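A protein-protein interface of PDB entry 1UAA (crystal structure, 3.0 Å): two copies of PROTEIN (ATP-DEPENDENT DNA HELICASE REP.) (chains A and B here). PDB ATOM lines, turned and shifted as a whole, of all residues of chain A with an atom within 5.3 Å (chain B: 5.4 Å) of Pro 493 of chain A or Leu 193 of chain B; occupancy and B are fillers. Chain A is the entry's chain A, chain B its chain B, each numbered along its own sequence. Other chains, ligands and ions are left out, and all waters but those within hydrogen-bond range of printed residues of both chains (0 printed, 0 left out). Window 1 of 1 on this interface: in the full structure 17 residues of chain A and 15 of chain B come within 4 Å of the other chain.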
ATOM      1  N   THR A 491      30.994 -17.191  -3.379  1.00  0.00           N
ATOM      2  CA  THR A 491      30.785 -15.764  -3.607  1.00  0.00           C
ATOM      3  C   THR A 491      29.316 -15.289  -3.652  1.00  0.00           C
ATOM      4  O   THR A 491      28.964 -14.227  -3.086  1.00  0.00           O
ATOM      5  CB  THR A 491      31.501 -15.316  -4.903  1.00  0.00           C
ATOM      6  OG1 THR A 491      31.153 -13.956  -5.227  1.00  0.00           O
ATOM      7  CG2 THR A 491      31.102 -16.192  -6.060  1.00  0.00           C
ATOM      8  N   SER A 492      28.484 -16.060  -4.356  1.00  0.00           N
ATOM      9  CA  SER A 492      27.064 -15.770  -4.537  1.00  0.00           C
ATOM     10  C   SER A 492      26.331 -15.783  -3.213  1.00  0.00           C
ATOM     11  O   SER A 492      26.654 -16.585  -2.326  1.00  0.00           O
ATOM     12  CB  SER A 492      26.414 -16.826  -5.430  1.00  0.00           C
ATOM     13  OG  SER A 492      27.076 -16.950  -6.673  1.00  0.00           O
ATOM     14  N   PRO A 493      25.339 -14.889  -3.057  1.00  0.00           N
ATOM     15  CA  PRO A 493      24.496 -14.730  -1.869  1.00  0.00           C
ATOM     16  C   PRO A 493      23.847 -16.063  -1.518  1.00  0.00           C
ATOM     17  O   PRO A 493      24.466 -16.952  -0.936  1.00  0.00           O
ATOM     18  CB  PRO A 493      23.461 -13.730  -2.350  1.00  0.00           C
ATOM     19  CG  PRO A 493      24.270 -12.842  -3.226  1.00  0.00           C
ATOM     20  CD  PRO A 493      25.098 -13.797  -4.017  1.00  0.00           C
ATOM     21  N   SER A 494      22.580 -16.201  -1.856  1.00  0.00           N
ATOM     22  CA  SER A 494      21.887 -17.457  -1.626  1.00  0.00           C
ATOM     23  C   SER A 494      22.552 -18.473  -2.546  1.00  0.00           C
ATOM     24  O   SER A 494      23.390 -18.121  -3.369  1.00  0.00           O
ATOM     25  CB  SER A 494      20.404 -17.311  -2.025  1.00  0.00           C
ATOM     26  OG  SER A 494      19.740 -18.566  -2.188  1.00  0.00           O
ATOM     27  N   PRO A 495      22.276 -19.753  -2.330  1.00  0.00           N
ATOM     28  CA  PRO A 495      22.840 -20.813  -3.157  1.00  0.00           C
ATOM     29  C   PRO A 495      22.181 -20.811  -4.529  1.00  0.00           C
ATOM     30  O   PRO A 495      22.855 -20.965  -5.554  1.00  0.00           O
ATOM     31  CB  PRO A 495      22.477 -22.059  -2.371  1.00  0.00           C
ATOM     32  CG  PRO A 495      22.567 -21.568  -0.965  1.00  0.00           C
ATOM     33  CD  PRO A 495      21.784 -20.302  -1.059  1.00  0.00           C
ATOM     34  N   ALA A 497      21.104 -18.400  -6.283  1.00  0.00           N
ATOM     35  CA  ALA A 497      21.677 -17.394  -7.183  1.00  0.00           C
ATOM     36  C   ALA A 497      22.936 -17.955  -7.813  1.00  0.00           C
ATOM     37  O   ALA A 497      23.192 -17.733  -8.986  1.00  0.00           O
ATOM     38  CB  ALA A 497      21.974 -16.103  -6.455  1.00  0.00           C
ATOM     39  N   ILE B  91      20.886  -3.749   1.594  1.00  0.00           N
ATOM     40  CA  ILE B  91      22.100  -4.380   1.117  1.00  0.00           C
ATOM     41  C   ILE B  91      21.568  -5.507   0.287  1.00  0.00           C
ATOM     42  O   ILE B  91      21.608  -5.431  -0.935  1.00  0.00           O
ATOM     43  CB  ILE B  91      22.934  -5.004   2.220  1.00  0.00           C
ATOM     44  CG1 ILE B  91      23.415  -3.960   3.234  1.00  0.00           C
ATOM     45  CG2 ILE B  91      24.121  -5.662   1.609  1.00  0.00           C
ATOM     46  CD1 ILE B  91      24.361  -2.908   2.668  1.00  0.00           C
ATOM     47  N   ILE B  92      20.929  -6.467   0.953  1.00  0.00           N
ATOM     48  CA  ILE B  92      20.378  -7.632   0.288  1.00  0.00           C
ATOM     49  C   ILE B  92      19.757  -7.264  -1.025  1.00  0.00           C
ATOM     50  O   ILE B  92      20.054  -7.879  -2.040  1.00  0.00           O
ATOM     51  CB  ILE B  92      19.358  -8.285   1.116  1.00  0.00           C
ATOM     52  CG1 ILE B  92      19.990  -8.763   2.390  1.00  0.00           C
ATOM     53  CG2 ILE B  92      18.868  -9.478   0.426  1.00  0.00           C
ATOM     54  CD1 ILE B  92      19.060  -8.706   3.507  1.00  0.00           C
ATOM     55  N   GLU B  95      22.628  -5.697  -3.661  1.00  0.00           N
ATOM     56  CA  GLU B  95      23.612  -6.621  -4.177  1.00  0.00           C
ATOM     57  C   GLU B  95      22.992  -7.783  -4.922  1.00  0.00           C
ATOM     58  O   GLU B  95      23.684  -8.466  -5.690  1.00  0.00           O
ATOM     59  CB  GLU B  95      24.588  -7.064  -3.094  1.00  0.00           C
ATOM     60  CG  GLU B  95      25.410  -5.912  -2.458  1.00  0.00           C
ATOM     61  CD  GLU B  95      26.288  -5.094  -3.430  1.00  0.00           C
ATOM     62  OE1 GLU B  95      25.847  -4.813  -4.564  1.00  0.00           O
ATOM     63  OE2 GLU B  95      27.404  -4.679  -3.029  1.00  0.00           O
ATOM     64  N   TYR B  96      21.688  -7.988  -4.716  1.00  0.00           N
ATOM     65  CA  TYR B  96      20.964  -9.033  -5.429  1.00  0.00           C
ATOM     66  C   TYR B  96      20.807  -8.515  -6.843  1.00  0.00           C
ATOM     67  O   TYR B  96      21.038  -9.241  -7.793  1.00  0.00           O
ATOM     68  CB  TYR B  96      19.618  -9.325  -4.788  1.00  0.00           C
ATOM     69  CG  TYR B  96      19.556 -10.726  -4.231  1.00  0.00           C
ATOM     70  CD1 TYR B  96      20.127 -11.053  -2.989  1.00  0.00           C
ATOM     71  CD2 TYR B  96      18.927 -11.730  -4.942  1.00  0.00           C
ATOM     72  CE1 TYR B  96      20.058 -12.369  -2.481  1.00  0.00           C
ATOM     73  CE2 TYR B  96      18.858 -13.026  -4.449  1.00  0.00           C
ATOM     74  CZ  TYR B  96      19.419 -13.346  -3.230  1.00  0.00           C
ATOM     75  OH  TYR B  96      19.319 -14.655  -2.817  1.00  0.00           O
ATOM     76  N   LEU B  99      24.286  -9.152  -9.164  1.00  0.00           N
ATOM     77  CA  LEU B  99      24.472 -10.386  -9.923  1.00  0.00           C
ATOM     78  C   LEU B  99      23.572 -10.360 -11.149  1.00  0.00           C
ATOM     79  O   LEU B  99      23.499 -11.321 -11.925  1.00  0.00           O
ATOM     80  CB  LEU B  99      24.053 -11.572  -9.076  1.00  0.00           C
ATOM     81  CG  LEU B  99      24.585 -11.646  -7.659  1.00  0.00           C
ATOM     82  CD1 LEU B  99      24.080 -12.934  -7.049  1.00  0.00           C
ATOM     83  CD2 LEU B  99      26.102 -11.599  -7.648  1.00  0.00           C
ATOM     84  N   LEU B 189      21.739 -11.380   7.029  1.00  0.00           N
ATOM     85  CA  LEU B 189      21.713 -11.670   5.625  1.00  0.00           C
ATOM     86  C   LEU B 189      22.934 -10.999   5.039  1.00  0.00           C
ATOM     87  O   LEU B 189      23.992 -11.588   5.040  1.00  0.00           O
ATOM     88  CB  LEU B 189      20.429 -11.131   5.029  1.00  0.00           C
ATOM     89  CG  LEU B 189      19.997 -12.036   3.913  1.00  0.00           C
ATOM     90  CD1 LEU B 189      20.928 -11.825   2.727  1.00  0.00           C
ATOM     91  CD2 LEU B 189      20.073 -13.482   4.458  1.00  0.00           C
ATOM     92  N   PRO B 190      22.860  -9.704   4.721  1.00  0.00           N
ATOM     93  CA  PRO B 190      24.079  -9.130   4.154  1.00  0.00           C
ATOM     94  C   PRO B 190      25.298  -9.406   5.005  1.00  0.00           C
ATOM     95  O   PRO B 190      26.384  -9.562   4.475  1.00  0.00           O
ATOM     96  CB  PRO B 190      23.783  -7.638   4.133  1.00  0.00           C
ATOM     97  CG  PRO B 190      22.381  -7.609   4.007  1.00  0.00           C
ATOM     98  CD  PRO B 190      21.930  -8.620   5.012  1.00  0.00           C
ATOM     99  N   THR B 191      25.108  -9.474   6.320  1.00  0.00           N
ATOM    100  CA  THR B 191      26.203  -9.747   7.234  1.00  0.00           C
ATOM    101  C   THR B 191      26.953 -10.896   6.573  1.00  0.00           C
ATOM    102  O   THR B 191      27.986 -10.656   5.968  1.00  0.00           O
ATOM    103  CB  THR B 191      25.649 -10.071   8.691  1.00  0.00           C
ATOM    104  OG1 THR B 191      25.577  -8.865   9.473  1.00  0.00           O
ATOM    105  CG2 THR B 191      26.502 -11.108   9.433  1.00  0.00           C
ATOM    106  N   LEU B 192      26.324 -12.064   6.475  1.00  0.00           N
ATOM    107  CA  LEU B 192      26.961 -13.218   5.842  1.00  0.00           C
ATOM    108  C   LEU B 192      27.401 -12.871   4.437  1.00  0.00           C
ATOM    109  O   LEU B 192      28.592 -12.780   4.161  1.00  0.00           O
ATOM    110  CB  LEU B 192      26.019 -14.419   5.778  1.00  0.00           C
ATOM    111  CG  LEU B 192      26.261 -15.484   6.861  1.00  0.00           C
ATOM    112  CD1 LEU B 192      25.647 -15.043   8.195  1.00  0.00           C
ATOM    113  CD2 LEU B 192      25.684 -16.840   6.443  1.00  0.00           C
ATOM    114  N   LEU B 193      26.436 -12.605   3.565  1.00  0.00           N
ATOM    115  CA  LEU B 193      26.741 -12.265   2.185  1.00  0.00           C
ATOM    116  C   LEU B 193      27.942 -11.314   2.062  1.00  0.00           C
ATOM    117  O   LEU B 193      28.622 -11.329   1.055  1.00  0.00           O
ATOM    118  CB  LEU B 193      25.505 -11.694   1.476  1.00  0.00           C
ATOM    119  CG  LEU B 193      25.733 -10.417   0.635  1.00  0.00           C
ATOM    120  CD1 LEU B 193      26.464 -10.735  -0.678  1.00  0.00           C
ATOM    121  CD2 LEU B 193      24.416  -9.729   0.331  1.00  0.00           C
ATOM    122  N   LEU B 194      28.215 -10.490   3.061  1.00  0.00           N
ATOM    123  CA  LEU B 194      29.358  -9.599   2.940  1.00  0.00           C
ATOM    124  C   LEU B 194      30.652 -10.182   3.485  1.00  0.00           C
ATOM    125  O   LEU B 194      31.750  -9.807   3.085  1.00  0.00           O
ATOM    126  CB  LEU B 194      29.087  -8.218   3.535  1.00  0.00           C
ATOM    127  CG  LEU B 194      28.429  -7.261   2.530  1.00  0.00           C
ATOM    128  CD1 LEU B 194      26.917  -7.488   2.564  1.00  0.00           C
ATOM    129  CD2 LEU B 194      28.773  -5.793   2.818  1.00  0.00           C
ATOM    130  N   GLN B 195      30.540 -11.099   4.420  1.00  0.00           N
ATOM    131  CA  GLN B 195      31.725 -11.725   4.967  1.00  0.00           C
ATOM    132  C   GLN B 195      32.229 -12.659   3.894  1.00  0.00           C
ATOM    133  O   GLN B 195      33.245 -12.385   3.290  1.00  0.00           O
ATOM    134  CB  GLN B 195      31.344 -12.495   6.226  1.00  0.00           C
ATOM    135  CG  GLN B 195      32.138 -13.752   6.505  1.00  0.00           C
ATOM    136  CD  GLN B 195      31.365 -14.710   7.407  1.00  0.00           C
ATOM    137  OE1 GLN B 195      31.660 -15.916   7.467  1.00  0.00           O
ATOM    138  NE2 GLN B 195      30.349 -14.179   8.100  1.00  0.00           N
ATOM    139  N   ALA B 196      31.403 -13.643   3.538  1.00  0.00           N
ATOM    140  CA  ALA B 196      31.730 -14.660   2.536  1.00  0.00           C
ATOM    141  C   ALA B 196      32.268 -14.147   1.206  1.00  0.00           C
ATOM    142  O   ALA B 196      33.065 -14.826   0.590  1.00  0.00           O
ATOM    143  CB  ALA B 196      30.518 -15.596   2.286  1.00  0.00           C
ATOM    144  N   ASN B 197      31.917 -12.927   0.807  1.00  0.00           N
ATOM    145  CA  ASN B 197      32.348 -12.391  -0.482  1.00  0.00           C
ATOM    146  C   ASN B 197      33.065 -11.075  -0.392  1.00  0.00           C
ATOM    147  O   ASN B 197      32.479 -10.091   0.029  1.00  0.00           O
ATOM    148  CB  ASN B 197      31.108 -12.236  -1.392  1.00  0.00           C
ATOM    149  CG  ASN B 197      31.307 -11.230  -2.549  1.00  0.00           C
ATOM    150  OD1 ASN B 197      31.654 -10.058  -2.330  1.00  0.00           O
ATOM    151  ND2 ASN B 197      31.012 -11.673  -3.776  1.00  0.00           N
ATOM    152  N   VAL B 200      31.781  -7.724  -3.099  1.00  0.00           N
ATOM    153  CA  VAL B 200      30.718  -6.886  -2.553  1.00  0.00           C
ATOM    154  C   VAL B 200      31.226  -6.074  -1.368  1.00  0.00           C
ATOM    155  O   VAL B 200      31.063  -4.850  -1.304  1.00  0.00           O
ATOM    156  CB  VAL B 200      29.534  -7.766  -2.054  1.00  0.00           C
ATOM    157  CG1 VAL B 200      28.525  -6.916  -1.306  1.00  0.00           C
ATOM    158  CG2 VAL B 200      28.863  -8.490  -3.215  1.00  0.00           C
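OG1 of Thr 491 of chain A lies within hydrogen-bond range of ND2 of Asn 197 of chain B.
N of Val 200 of chain B is in hydrogen-bond range of OD1 of Asn 197 of chain B (2.5 Å).
Pro 493 of chain A touches Tyr 96 of chain B.
Pro 493 of chain A touches Leu 99 of chain B.
CG of Pro 493 of chain A touches CD1 of Leu 193 of chain B, 3.97 Å away.
Ser 494 of chain A touches Tyr 96 of chain B.
Ala 497 of chain A touches Leu 99 of chain B (CB to CD1, 3.9 Å).
Of the printed residues of chain B, Pro 493 of chain A touches Tyr 96 (3.7 Å), Leu 99 (3.3 Å) and Leu 193 (3.97 Å).
Leu 193 of chain B touches one residue of chain A.
Of the printed residues of chain A, Asn 197 of chain B touches Thr 491.
Of the printed residues of chain A, Tyr 96 of chain B touches Pro 493 (3.7 Å) and Ser 494 (3.0 Å).
Of the printed residues of chain B, Ser 494 of chain A touches Tyr 96 (3.0 Å).
Printed residues of chain A within 4 Å of Leu 99 of chain B: Pro 493 and Ala 497.
Thr 191 of chain B touches none of the printed residues of chain A.
The nearest residue of chain B that does not touch Pro 493 of chain A is Glu 95 of chain B (5.1 Å).
The nearest printed residue of chain A that does not touch Tyr 96 of chain B is Ala 497 of chain A (4.7 Å).
Hydrophobic or aromatic side chains of chain B within 4 Å of the printed part of chain A: Tyr 96, Leu 99 and Leu 193.
Printed residues of chain A that touch a printed residue of chain B: Thr 491, Pro 493, Ser 494 and Ala 497.
Among the printed residues, 6 pairs touch across the chains.
Among the printed residues, no Asp or Glu carboxylate lies within 4 Å of a Lys or Arg side-chain nitrogen of the other chain.
No position is printed for both chains.
Of the 6 pairs that touch across the chains among the printed residues, none has its exchanged pair printed and touching as well.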
